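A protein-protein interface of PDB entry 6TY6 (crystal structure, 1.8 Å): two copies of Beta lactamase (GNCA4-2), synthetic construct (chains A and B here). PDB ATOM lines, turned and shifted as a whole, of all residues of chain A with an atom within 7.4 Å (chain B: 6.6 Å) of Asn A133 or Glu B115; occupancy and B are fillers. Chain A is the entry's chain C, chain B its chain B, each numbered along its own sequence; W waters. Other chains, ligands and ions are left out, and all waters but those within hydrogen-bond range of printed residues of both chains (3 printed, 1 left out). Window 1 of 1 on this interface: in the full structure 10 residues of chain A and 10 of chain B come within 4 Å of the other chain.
Water W1 bridges NH1 of Arg B68 (2.9 Å) and O of Asn A133 (2.9 Å).
Water W3 bridges OE1 of Glu B115 and NE of Arg A40.
Water W2 bridges the side-chain carboxylate of Glu B115 (3.0 Å) and the guanidinium group of Arg A40 (3.0 Å).
Among the printed residues, pairs that only touch across the chains: Asn A133 with Arg B68, Asn A133 with Ala B116, Arg A128 with Gly B118, Arg A128 with Leu B117, Pro A152 with Glu B115, Val A134 with Arg B68, Asn A133 with Glu B115, Thr A124 with Gly B118, Gly A131 with Lys B63 and Arg A136 with Trp B140.
The backbone carbonyl oxygen (O) of Arg A128 lies within hydrogen-bond range of the guanidinium group (NH2) of Arg B58 (2.9 Å).
ND2 of Asn A133 is in hydrogen-bond range of OE2 of Glu B64 (3.3 Å).
O of Ala B116 lies within hydrogen-bond range of NE of Arg A128 (2.9 Å).
The guanidinium group (NH1) of Arg A136 lies within salt-bridge range of the side-chain carboxylate (OE2) of Glu B115.
The backbone carbonyl oxygen (O) of Glu B115 is in hydrogen-bond range of the guanidinium group (NH2) of Arg A128, at 2.8 Å.
The guanidinium group (NH2) of Arg B58 lies within hydrogen-bond range of the side-chain amide oxygen (OD1) of Asn A133.
The guanidinium group (NE) of Arg A40 lies within salt-bridge range of the side-chain carboxylate (OE2) of Glu B115, 3.5 Å away.
The side-chain amino group (NZ) of Lys B63 sits at hydrogen-bond distance from the backbone carbonyl oxygen (O) of Ser A129, at 2.8 Å.
The backbone carbonyl oxygen (O) of Lys B63 lies within hydrogen-bond range of the side-chain amide nitrogen (ND2) of Asn A133 (2.8 Å).
Printed residues of chain B that touch a printed residue of chain A: Arg B58, Lys B63, Glu B64, Arg B68, Glu B115, Ala B116, Leu B117, Gly B118 and Trp B140.
Hydrophobic or aromatic side chains of chain B that line the printed part of chain A: Trp B140.
Of the 19 printed residues of chain A, 9 touch a printed residue of chain B.
Among the printed residues, Asp or Glu carboxylates within 4 Å of a Lys or Arg side-chain nitrogen of the other chain: Arg A40 with Glu B115 (3.5 Å) and Arg A136 with Glu B115 (2.8 Å).
Printed residues of chain B within 4 Å of Arg A40: Glu B115.
Asn A133 touches just these residues of chain B: Arg B58 (2.7 Å), Lys B63 (2.8 Å), Glu B64 (3.3 Å), Arg B68 (3.3 Å), Glu B115 (3.8 Å) and Ala B116 (3.5 Å).
Of the printed residues of chain A, Lys B63 touches Ser A129 (2.8 Å), Gly A131 (3.9 Å) and Asn A133 (2.8 Å).
Printed residues of chain A within 4 Å of Glu B115: Arg A40 (3.4 Å), Arg A128 (2.8 Å), Asn A133 (3.8 Å), Arg A136 (2.8 Å) and Pro A152 (3.6 Å).
Gly B119 touches none of the printed residues of chain A.
Of the printed residues of chain A, Trp B140 touches Arg A136.
The nearest residue of chain B that does not touch Asn A133 is Asn B65 (5.0 Å).
No position is printed for both chains.
NH1 of Arg A128 is in hydrogen-bond range of O of Thr A135, 2.8 Å away.
O of Arg B58 is in hydrogen-bond range of N of Glu B64 (3.3 Å).
O of Thr A155 is in hydrogen-bond range of N of Arg A136 (3.1 Å).
NE of Arg A136 lies within salt-bridge range of OD2 of Asp A138 (2.8 Å).
The backbone carbonyl oxygen of Arg B58 is in hydrogen-bond range of the backbone NH of Lys B63, 2.9 Å away.
OG1 of Thr A155 lies within hydrogen-bond range of O of Pro A152 (2.6 Å).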
ATOM      1  N   ARG A  40      17.843  23.782   1.800  1.00  0.00           N
ATOM      2  CA  ARG A  40      17.168  23.812   3.098  1.00  0.00           C
ATOM      3  C   ARG A  40      16.465  25.151   3.331  1.00  0.00           C
ATOM      4  O   ARG A  40      16.995  26.220   2.987  1.00  0.00           O
ATOM      5  CB  ARG A  40      18.160  23.585   4.236  1.00  0.00           C
ATOM      6  CG  ARG A  40      18.757  22.165   4.261  1.00  0.00           C
ATOM      7  CD  ARG A  40      19.379  21.770   5.646  1.00  0.00           C
ATOM      8  NE  ARG A  40      19.704  20.357   5.639  1.00  0.00           N
ATOM      9  CZ  ARG A  40      18.898  19.429   6.153  1.00  0.00           C
ATOM     10  NH1 ARG A  40      17.746  19.767   6.711  1.00  0.00           N
ATOM     11  NH2 ARG A  40      19.209  18.164   6.048  1.00  0.00           N
ATOM     12  N   THR A 124      12.140  13.733  14.671  1.00  0.00           N
ATOM     13  CA  THR A 124      13.162  13.469  13.679  1.00  0.00           C
ATOM     14  C   THR A 124      13.367  11.959  13.482  1.00  0.00           C
ATOM     15  O   THR A 124      13.502  11.493  12.335  1.00  0.00           O
ATOM     16  CB  THR A 124      14.439  14.195  14.092  1.00  0.00           C
ATOM     17  OG1 THR A 124      14.198  15.612  14.134  1.00  0.00           O
ATOM     18  CG2 THR A 124      15.565  13.925  13.175  1.00  0.00           C
ATOM     19  N   LEU A 127      10.698  10.569  11.252  1.00  0.00           N
ATOM     20  CA  LEU A 127      10.931  10.853   9.823  1.00  0.00           C
ATOM     21  C   LEU A 127      12.017   9.921   9.280  1.00  0.00           C
ATOM     22  O   LEU A 127      11.873   9.356   8.171  1.00  0.00           O
ATOM     23  CB  LEU A 127      11.331  12.306   9.662  1.00  0.00           C
ATOM     24  CG  LEU A 127      10.113  13.209  10.084  1.00  0.00           C
ATOM     25  CD1 LEU A 127      10.551  14.657  10.148  1.00  0.00           C
ATOM     26  CD2 LEU A 127       8.930  13.022   9.065  1.00  0.00           C
ATOM     27  N   ARG A 128      13.077   9.721  10.059  1.00  0.00           N
ATOM     28  CA  ARG A 128      14.099   8.801   9.580  1.00  0.00           C
ATOM     29  C   ARG A 128      13.513   7.401   9.466  1.00  0.00           C
ATOM     30  O   ARG A 128      13.883   6.652   8.568  1.00  0.00           O
ATOM     31  CB  ARG A 128      15.327   8.811  10.505  1.00  0.00           C
ATOM     32  CG  ARG A 128      16.139  10.114  10.513  1.00  0.00           C
ATOM     33  CD  ARG A 128      16.717  10.517   9.162  1.00  0.00           C
ATOM     34  NE  ARG A 128      17.394  11.814   9.266  1.00  0.00           N
ATOM     35  CZ  ARG A 128      16.717  12.978   9.274  1.00  0.00           C
ATOM     36  NH1 ARG A 128      15.386  12.945   9.151  1.00  0.00           N
ATOM     37  NH2 ARG A 128      17.348  14.153   9.410  1.00  0.00           N
ATOM     38  N   SER A 129      12.550   7.046  10.327  1.00  0.00           N
ATOM     39  CA  SER A 129      12.045   5.692  10.202  1.00  0.00           C
ATOM     40  C   SER A 129      11.220   5.499   8.922  1.00  0.00           C
ATOM     41  O   SER A 129      10.970   4.352   8.538  1.00  0.00           O
ATOM     42  CB  SER A 129      11.241   5.306  11.421  1.00  0.00           C
ATOM     43  OG  SER A 129       9.868   5.822  11.328  1.00  0.00           O
ATOM     44  N   ILE A 130      10.838   6.563   8.220  1.00  0.00           N
ATOM     45  CA  ILE A 130      10.051   6.408   7.000  1.00  0.00           C
ATOM     46  C   ILE A 130      10.851   6.821   5.793  1.00  0.00           C
ATOM     47  O   ILE A 130      10.300   6.948   4.699  1.00  0.00           O
ATOM     48  CB  ILE A 130       8.690   7.167   7.073  1.00  0.00           C
ATOM     49  CG1 ILE A 130       8.870   8.701   7.142  1.00  0.00           C
ATOM     50  CG2 ILE A 130       7.878   6.669   8.242  1.00  0.00           C
ATOM     51  CD1 ILE A 130       7.466   9.504   7.111  1.00  0.00           C
ATOM     52  N   GLY A 131      12.167   7.007   5.963  1.00  0.00           N
ATOM     53  CA  GLY A 131      13.027   7.251   4.834  1.00  0.00           C
ATOM     54  C   GLY A 131      13.203   8.688   4.403  1.00  0.00           C
ATOM     55  O   GLY A 131      13.644   8.916   3.279  1.00  0.00           O
ATOM     56  N   ASP A 132      12.820   9.658   5.218  1.00  0.00           N
ATOM     57  CA  ASP A 132      13.081  11.081   4.965  1.00  0.00           C
ATOM     58  C   ASP A 132      14.366  11.335   5.696  1.00  0.00           C
ATOM     59  O   ASP A 132      14.420  11.309   6.957  1.00  0.00           O
ATOM     60  CB  ASP A 132      11.944  11.954   5.497  1.00  0.00           C
ATOM     61  CG  ASP A 132      12.213  13.486   5.386  1.00  0.00           C
ATOM     62  OD1 ASP A 132      13.390  13.937   5.273  1.00  0.00           O
ATOM     63  OD2 ASP A 132      11.183  14.270   5.528  1.00  0.00           O
ATOM     64  N   ASN A 133      15.444  11.385   4.940  1.00  0.00           N
ATOM     65  CA  ASN A 133      16.739  11.498   5.569  1.00  0.00           C
ATOM     66  C   ASN A 133      17.173  12.938   5.675  1.00  0.00           C
ATOM     67  O   ASN A 133      18.354  13.195   5.953  1.00  0.00           O
ATOM     68  CB  ASN A 133      17.778  10.639   4.839  1.00  0.00           C
ATOM     69  CG  ASN A 133      17.406   9.176   4.890  1.00  0.00           C
ATOM     70  OD1 ASN A 133      17.087   8.674   5.959  1.00  0.00           O
ATOM     71  ND2 ASN A 133      17.385   8.501   3.760  1.00  0.00           N
ATOM     72  N   VAL A 134      16.224  13.893   5.554  1.00  0.00           N
ATOM     73  CA  VAL A 134      16.575  15.273   5.282  1.00  0.00           C
ATOM     74  C   VAL A 134      15.993  16.212   6.316  1.00  0.00           C
ATOM     75  O   VAL A 134      16.718  17.054   6.874  1.00  0.00           O
ATOM     76  CB  VAL A 134      16.130  15.708   3.850  1.00  0.00           C
ATOM     77  CG1 VAL A 134      16.269  17.181   3.719  1.00  0.00           C
ATOM     78  CG2 VAL A 134      16.965  15.048   2.844  1.00  0.00           C
ATOM     79  N   THR A 135      14.664  16.141   6.521  1.00  0.00           N
ATOM     80  CA  THR A 135      13.950  16.990   7.456  1.00  0.00           C
ATOM     81  C   THR A 135      14.439  16.752   8.885  1.00  0.00           C
ATOM     82  O   THR A 135      14.751  15.619   9.284  1.00  0.00           O
ATOM     83  CB  THR A 135      12.446  16.689   7.382  1.00  0.00           C
ATOM     84  OG1 THR A 135      12.019  16.750   6.020  1.00  0.00           O
ATOM     85  CG2 THR A 135      11.605  17.700   8.183  1.00  0.00           C
ATOM     86  N   ARG A 136      14.497  17.826   9.666  1.00  0.00           N
ATOM     87  CA  ARG A 136      14.946  17.702  11.041  1.00  0.00           C
ATOM     88  C   ARG A 136      14.222  18.713  11.898  1.00  0.00           C
ATOM     89  O   ARG A 136      14.139  19.888  11.528  1.00  0.00           O
ATOM     90  CB  ARG A 136      16.462  17.935  11.198  1.00  0.00           C
ATOM     91  CG  ARG A 136      16.966  19.250  10.495  1.00  0.00           C
ATOM     92  CD  ARG A 136      18.525  19.352  10.579  1.00  0.00           C
ATOM     93  NE  ARG A 136      18.962  19.698  11.935  1.00  0.00           N
ATOM     94  CZ  ARG A 136      20.220  19.989  12.268  1.00  0.00           C
ATOM     95  NH1 ARG A 136      21.175  19.879  11.355  1.00  0.00           N
ATOM     96  NH2 ARG A 136      20.518  20.368  13.511  1.00  0.00           N
ATOM     97  N   ASP A 138      14.472  20.312  15.842  1.00  0.00           N
ATOM     98  CA  ASP A 138      15.575  20.508  16.769  1.00  0.00           C
ATOM     99  C   ASP A 138      15.100  21.183  18.014  1.00  0.00           C
ATOM    100  O   ASP A 138      15.619  20.880  19.092  1.00  0.00           O
ATOM    101  CB  ASP A 138      16.665  21.372  16.149  1.00  0.00           C
ATOM    102  CG  ASP A 138      17.436  20.634  15.116  1.00  0.00           C
ATOM    103  OD1 ASP A 138      18.380  19.941  15.555  1.00  0.00           O
ATOM    104  OD2 ASP A 138      17.158  20.727  13.883  1.00  0.00           O
ATOM    105  N   ASP A 151      21.255  28.571   9.350  1.00  0.00           N
ATOM    106  CA  ASP A 151      21.068  27.706  10.515  1.00  0.00           C
ATOM    107  C   ASP A 151      20.281  26.482  10.058  1.00  0.00           C
ATOM    108  O   ASP A 151      19.128  26.634   9.653  1.00  0.00           O
ATOM    109  CB  ASP A 151      20.308  28.461  11.595  1.00  0.00           C
ATOM    110  CG  ASP A 151      20.106  27.645  12.890  1.00  0.00           C
ATOM    111  OD1 ASP A 151      20.451  26.443  12.948  1.00  0.00           O
ATOM    112  OD2 ASP A 151      19.554  28.259  13.833  1.00  0.00           O
ATOM    113  N   PRO A 152      20.849  25.283  10.055  1.00  0.00           N
ATOM    114  CA  PRO A 152      20.091  24.127   9.546  1.00  0.00           C
ATOM    115  C   PRO A 152      19.053  23.583  10.502  1.00  0.00           C
ATOM    116  O   PRO A 152      18.340  22.643  10.115  1.00  0.00           O
ATOM    117  CB  PRO A 152      21.185  23.060   9.330  1.00  0.00           C
ATOM    118  CG  PRO A 152      22.192  23.403  10.361  1.00  0.00           C
ATOM    119  CD  PRO A 152      22.240  24.907  10.417  1.00  0.00           C
ATOM    120  N   ARG A 153      19.012  24.038  11.758  1.00  0.00           N
ATOM    121  CA  ARG A 153      18.020  23.519  12.682  1.00  0.00           C
ATOM    122  C   ARG A 153      16.629  23.760  12.110  1.00  0.00           C
ATOM    123  O   ARG A 153      16.400  24.766  11.429  1.00  0.00           O
ATOM    124  CB  ARG A 153      18.132  24.202  14.042  1.00  0.00           C
ATOM    125  CG  ARG A 153      19.452  23.785  14.785  1.00  0.00           C
ATOM    126  CD  ARG A 153      19.569  24.560  16.086  1.00  0.00           C
ATOM    127  NE  ARG A 153      19.844  25.981  15.850  1.00  0.00           N
ATOM    128  CZ  ARG A 153      19.948  26.853  16.843  1.00  0.00           C
ATOM    129  NH1 ARG A 153      19.822  26.415  18.079  1.00  0.00           N
ATOM    130  NH2 ARG A 153      20.178  28.135  16.618  1.00  0.00           N
ATOM    131  N   THR A 155      14.772  22.641   9.747  1.00  0.00           N
ATOM    132  CA  THR A 155      14.646  22.874   8.306  1.00  0.00           C
ATOM    133  C   THR A 155      14.145  21.612   7.622  1.00  0.00           C
ATOM    134  O   THR A 155      14.141  20.516   8.183  1.00  0.00           O
ATOM    135  CB  THR A 155      15.976  23.293   7.642  1.00  0.00           C
ATOM    136  OG1 THR A 155      17.027  22.284   7.928  1.00  0.00           O
ATOM    137  CG2 THR A 155      16.383  24.632   8.177  1.00  0.00           C
ATOM    138  N   ALA A 160      12.022  17.347  -0.203  1.00  0.00           N
ATOM    139  CA  ALA A 160      11.876  16.348   0.881  1.00  0.00           C
ATOM    140  C   ALA A 160      10.469  16.423   1.484  1.00  0.00           C
ATOM    141  O   ALA A 160       9.783  15.397   1.656  1.00  0.00           O
ATOM    142  CB  ALA A 160      12.964  16.562   1.940  1.00  0.00           C
ATOM    143  N   THR A 164       7.719  13.477   1.464  1.00  0.00           N
ATOM    144  CA  THR A 164       7.283  12.911   2.745  1.00  0.00           C
ATOM    145  C   THR A 164       5.770  13.057   2.924  1.00  0.00           C
ATOM    146  O   THR A 164       5.085  12.121   3.393  1.00  0.00           O
ATOM    147  CB  THR A 164       8.015  13.603   3.880  1.00  0.00           C
ATOM    148  OG1 THR A 164       9.421  13.171   3.812  1.00  0.00           O
ATOM    149  CG2 THR A 164       7.436  13.135   5.254  1.00  0.00           C
ATOM    150  N   LEU B  51      30.067   6.194  12.356  1.00  0.00           N
ATOM    151  CA  LEU B  51      29.078   6.995  11.603  1.00  0.00           C
ATOM    152  C   LEU B  51      28.807   6.320  10.260  1.00  0.00           C
ATOM    153  O   LEU B  51      27.660   6.081   9.892  1.00  0.00           O
ATOM    154  CB  LEU B  51      29.660   8.414  11.431  1.00  0.00           C
ATOM    155  CG  LEU B  51      28.937   9.383  10.482  1.00  0.00           C
ATOM    156  CD1 LEU B  51      27.513   9.689  11.053  1.00  0.00           C
ATOM    157  CD2 LEU B  51      29.688  10.646  10.280  1.00  0.00           C
ATOM    158  N   ARG B  58      21.452   1.626   7.633  1.00  0.00           N
ATOM    159  CA  ARG B  58      20.176   2.142   7.095  1.00  0.00           C
ATOM    160  C   ARG B  58      20.051   1.842   5.603  1.00  0.00           C
ATOM    161  O   ARG B  58      18.939   1.600   5.092  1.00  0.00           O
ATOM    162  CB  ARG B  58      20.026   3.656   7.362  1.00  0.00           C
ATOM    163  CG  ARG B  58      20.005   3.994   8.823  1.00  0.00           C
ATOM    164  CD  ARG B  58      19.834   5.500   9.130  1.00  0.00           C
ATOM    165  NE  ARG B  58      18.786   6.164   8.317  1.00  0.00           N
ATOM    166  CZ  ARG B  58      17.466   6.075   8.511  1.00  0.00           C
ATOM    167  NH1 ARG B  58      16.939   5.345   9.487  1.00  0.00           N
ATOM    168  NH2 ARG B  58      16.665   6.715   7.694  1.00  0.00           N
ATOM    169  N   LYS B  63      16.299   2.226   4.132  1.00  0.00           N
ATOM    170  CA  LYS B  63      15.888   3.579   4.506  1.00  0.00           C
ATOM    171  C   LYS B  63      16.855   4.649   4.004  1.00  0.00           C
ATOM    172  O   LYS B  63      16.571   5.843   4.123  1.00  0.00           O
ATOM    173  CB  LYS B  63      15.752   3.669   6.027  1.00  0.00           C
ATOM    174  CG  LYS B  63      14.621   2.823   6.585  1.00  0.00           C
ATOM    175  CD  LYS B  63      14.760   2.754   8.098  1.00  0.00           C
ATOM    176  CE  LYS B  63      13.878   1.676   8.736  1.00  0.00           C
ATOM    177  NZ  LYS B  63      12.453   1.987   8.426  1.00  0.00           N
ATOM    178  N   GLU B  64      17.982   4.239   3.440  1.00  0.00           N
ATOM    179  CA  GLU B  64      18.986   5.150   2.940  1.00  0.00           C
ATOM    180  C   GLU B  64      19.492   4.574   1.625  1.00  0.00           C
ATOM    181  O   GLU B  64      19.371   3.376   1.364  1.00  0.00           O
ATOM    182  CB  GLU B  64      20.073   5.326   3.993  1.00  0.00           C
ATOM    183  CG  GLU B  64      21.212   6.289   3.678  1.00  0.00           C
ATOM    184  CD  GLU B  64      20.690   7.708   3.370  1.00  0.00           C
ATOM    185  OE1 GLU B  64      20.319   7.899   2.182  1.00  0.00           O
ATOM    186  OE2 GLU B  64      20.651   8.586   4.305  1.00  0.00           O
ATOM    187  N   ASN B  65      20.035   5.429   0.781  1.00  0.00           N
ATOM    188  CA  ASN B  65      20.542   5.020  -0.517  1.00  0.00           C
ATOM    189  C   ASN B  65      21.936   5.610  -0.706  1.00  0.00           C
ATOM    190  O   ASN B  65      22.103   6.814  -0.505  1.00  0.00           O
ATOM    191  CB  ASN B  65      19.594   5.495  -1.624  1.00  0.00           C
ATOM    192  CG  ASN B  65      19.863   4.805  -2.919  1.00  0.00           C
ATOM    193  OD1 ASN B  65      21.014   4.692  -3.347  1.00  0.00           O
ATOM    194  ND2 ASN B  65      18.808   4.343  -3.572  1.00  0.00           N
ATOM    195  N   ARG B  68      22.220   8.551  -3.030  1.00  0.00           N
ATOM    196  CA  ARG B  68      21.354   9.720  -2.796  1.00  0.00           C
ATOM    197  C   ARG B  68      22.227  10.958  -2.684  1.00  0.00           C
ATOM    198  O   ARG B  68      23.175  10.985  -1.889  1.00  0.00           O
ATOM    199  CB  ARG B  68      20.529   9.593  -1.528  1.00  0.00           C
ATOM    200  CG  ARG B  68      19.835  10.907  -1.114  1.00  0.00           C
ATOM    201  CD  ARG B  68      18.968  10.643   0.063  1.00  0.00           C
ATOM    202  NE  ARG B  68      19.671  10.470   1.354  1.00  0.00           N
ATOM    203  CZ  ARG B  68      20.052  11.461   2.169  1.00  0.00           C
ATOM    204  NH1 ARG B  68      19.830  12.749   1.818  1.00  0.00           N
ATOM    205  NH2 ARG B  68      20.678  11.178   3.322  1.00  0.00           N
ATOM    206  N   ILE B  70      23.401  14.784  -1.897  1.00  0.00           N
ATOM    207  CA  ILE B  70      23.160  15.745  -0.826  1.00  0.00           C
ATOM    208  C   ILE B  70      23.797  17.075  -1.224  1.00  0.00           C
ATOM    209  O   ILE B  70      24.981  17.126  -1.557  1.00  0.00           O
ATOM    210  CB  ILE B  70      23.708  15.245   0.533  1.00  0.00           C
ATOM    211  CG1 ILE B  70      22.891  14.088   1.054  1.00  0.00           C
ATOM    212  CG2 ILE B  70      23.691  16.377   1.580  1.00  0.00           C
ATOM    213  CD1 ILE B  70      23.397  13.591   2.436  1.00  0.00           C
ATOM    214  N   VAL B  94      25.726  10.138  -0.680  1.00  0.00           N
ATOM    215  CA  VAL B  94      25.922   9.473   0.601  1.00  0.00           C
ATOM    216  C   VAL B  94      27.229   8.676   0.561  1.00  0.00           C
ATOM    217  O   VAL B  94      28.102   8.837   1.412  1.00  0.00           O
ATOM    218  CB  VAL B  94      24.721   8.574   0.922  1.00  0.00           C
ATOM    219  CG1 VAL B  94      25.013   7.698   2.145  1.00  0.00           C
ATOM    220  CG2 VAL B  94      23.404   9.425   1.322  1.00  0.00           C
ATOM    221  N   ALA B 110      31.162  14.580   7.614  1.00  0.00           N
ATOM    222  CA  ALA B 110      30.658  13.916   8.814  1.00  0.00           C
ATOM    223  C   ALA B 110      29.378  14.603   9.301  1.00  0.00           C
ATOM    224  O   ALA B 110      28.439  13.925   9.747  1.00  0.00           O
ATOM    225  CB  ALA B 110      31.736  13.923   9.891  1.00  0.00           C
ATOM    226  N   ASN B 111      29.340  15.933   9.272  1.00  0.00           N
ATOM    227  CA  ASN B 111      28.108  16.630   9.716  1.00  0.00           C
ATOM    228  C   ASN B 111      26.949  16.279   8.807  1.00  0.00           C
ATOM    229  O   ASN B 111      25.814  16.092   9.269  1.00  0.00           O
ATOM    230  CB  ASN B 111      28.284  18.155   9.721  1.00  0.00           C
ATOM    231  CG  ASN B 111      28.946  18.648  10.993  1.00  0.00           C
ATOM    232  OD1 ASN B 111      29.061  17.903  12.005  1.00  0.00           O
ATOM    233  ND2 ASN B 111      29.439  19.881  10.935  1.00  0.00           N
ATOM    234  N   LEU B 112      27.184  16.335   7.485  1.00  0.00           N
ATOM    235  CA  LEU B 112      26.100  16.021   6.563  1.00  0.00           C
ATOM    236  C   LEU B 112      25.594  14.617   6.830  1.00  0.00           C
ATOM    237  O   LEU B 112      24.382  14.385   6.843  1.00  0.00           O
ATOM    238  CB  LEU B 112      26.542  16.162   5.098  1.00  0.00           C
ATOM    239  CG  LEU B 112      26.906  17.567   4.686  1.00  0.00           C
ATOM    240  CD1 LEU B 112      27.532  17.508   3.314  1.00  0.00           C
ATOM    241  CD2 LEU B 112      25.606  18.476   4.634  1.00  0.00           C
ATOM    242  N   LEU B 113      26.514  13.674   7.096  1.00  0.00           N
ATOM    243  CA  LEU B 113      26.088  12.308   7.389  1.00  0.00           C
ATOM    244  C   LEU B 113      25.383  12.215   8.733  1.00  0.00           C
ATOM    245  O   LEU B 113      24.441  11.422   8.891  1.00  0.00           O
ATOM    246  CB  LEU B 113      27.311  11.318   7.382  1.00  0.00           C
ATOM    247  CG  LEU B 113      27.836  11.145   5.966  1.00  0.00           C
ATOM    248  CD1 LEU B 113      29.258  10.361   6.020  1.00  0.00           C
ATOM    249  CD2 LEU B 113      26.877  10.374   5.119  1.00  0.00           C
ATOM    250  N   LEU B 114      25.861  12.955   9.745  1.00  0.00           N
ATOM    251  CA  LEU B 114      25.116  12.974  11.007  1.00  0.00           C
ATOM    252  C   LEU B 114      23.681  13.481  10.754  1.00  0.00           C
ATOM    253  O   LEU B 114      22.708  12.952  11.296  1.00  0.00           O
ATOM    254  CB  LEU B 114      25.817  13.879  12.022  1.00  0.00           C
ATOM    255  CG  LEU B 114      27.016  13.210  12.717  1.00  0.00           C
ATOM    256  CD1 LEU B 114      27.901  14.289  13.351  1.00  0.00           C
ATOM    257  CD2 LEU B 114      26.518  12.241  13.818  1.00  0.00           C
ATOM    258  N   GLU B 115      23.542  14.451   9.860  1.00  0.00           N
ATOM    259  CA  GLU B 115      22.199  14.963   9.617  1.00  0.00           C
ATOM    260  C   GLU B 115      21.323  13.884   8.978  1.00  0.00           C
ATOM    261  O   GLU B 115      20.139  13.755   9.304  1.00  0.00           O
ATOM    262  CB  GLU B 115      22.295  16.159   8.677  1.00  0.00           C
ATOM    263  CG  GLU B 115      22.396  17.477   9.352  1.00  0.00           C
ATOM    264  CD  GLU B 115      22.097  18.565   8.300  1.00  0.00           C
ATOM    265  OE1 GLU B 115      22.610  18.388   7.170  1.00  0.00           O
ATOM    266  OE2 GLU B 115      21.284  19.502   8.586  1.00  0.00           O
ATOM    267  N   ALA B 116      21.917  13.092   8.070  1.00  0.00           N
ATOM    268  CA  ALA B 116      21.223  11.972   7.446  1.00  0.00           C
ATOM    269  C   ALA B 116      20.747  10.946   8.482  1.00  0.00           C
ATOM    270  O   ALA B 116      19.667  10.351   8.290  1.00  0.00           O
ATOM    271  CB  ALA B 116      22.137  11.275   6.413  1.00  0.00           C
ATOM    272  N   LEU B 117      21.467  10.800   9.614  1.00  0.00           N
ATOM    273  CA  LEU B 117      20.961   9.926  10.690  1.00  0.00           C
ATOM    274  C   LEU B 117      19.946  10.624  11.594  1.00  0.00           C
ATOM    275  O   LEU B 117      19.252   9.932  12.350  1.00  0.00           O
ATOM    276  CB  LEU B 117      22.054   9.448  11.632  1.00  0.00           C
ATOM    277  CG  LEU B 117      23.243   8.657  11.074  1.00  0.00           C
ATOM    278  CD1 LEU B 117      24.170   8.283  12.300  1.00  0.00           C
ATOM    279  CD2 LEU B 117      22.709   7.457  10.257  1.00  0.00           C
ATOM    280  N   GLY B 118      19.973  11.958  11.660  1.00  0.00           N
ATOM    281  CA  GLY B 118      19.167  12.715  12.613  1.00  0.00           C
ATOM    282  C   GLY B 118      19.966  13.213  13.808  1.00  0.00           C
ATOM    283  O   GLY B 118      19.389  13.803  14.718  1.00  0.00           O
ATOM    284  N   GLY B 119      21.280  13.085  13.794  1.00  0.00           N
ATOM    285  CA  GLY B 119      22.090  13.818  14.759  1.00  0.00           C
ATOM    286  C   GLY B 119      22.959  12.880  15.651  1.00  0.00           C
ATOM    287  O   GLY B 119      22.858  11.647  15.554  1.00  0.00           O
ATOM    288  N   TRP B 140      28.414  18.028  17.336  1.00  0.00           N
ATOM    289  CA  TRP B 140      28.728  18.048  15.921  1.00  0.00           C
ATOM    290  C   TRP B 140      30.183  18.497  15.679  1.00  0.00           C
ATOM    291  O   TRP B 140      30.925  18.850  16.601  1.00  0.00           O
ATOM    292  CB  TRP B 140      27.778  19.010  15.194  1.00  0.00           C
ATOM    293  CG  TRP B 140      26.306  18.682  15.332  1.00  0.00           C
ATOM    294  CD1 TRP B 140      25.508  18.931  16.393  1.00  0.00           C
ATOM    295  CD2 TRP B 140      25.470  18.071  14.333  1.00  0.00           C
ATOM    296  NE1 TRP B 140      24.210  18.503  16.134  1.00  0.00           N
ATOM    297  CE2 TRP B 140      24.158  18.003  14.860  1.00  0.00           C
ATOM    298  CE3 TRP B 140      25.693  17.612  13.031  1.00  0.00           C
ATOM    299  CZ2 TRP B 140      23.095  17.447  14.148  1.00  0.00           C
ATOM    300  CZ3 TRP B 140      24.610  17.085  12.304  1.00  0.00           C
ATOM    301  CH2 TRP B 140      23.337  17.020  12.864  1.00  0.00           C
HETATM  302  O   HOH W   1      20.568  14.023   4.291  1.00  0.00           O
HETATM  303  O   HOH W   2      21.683  18.265   4.279  1.00  0.00           O
HETATM  304  O   HOH W   3      23.063  20.855   5.524  1.00  0.00           O
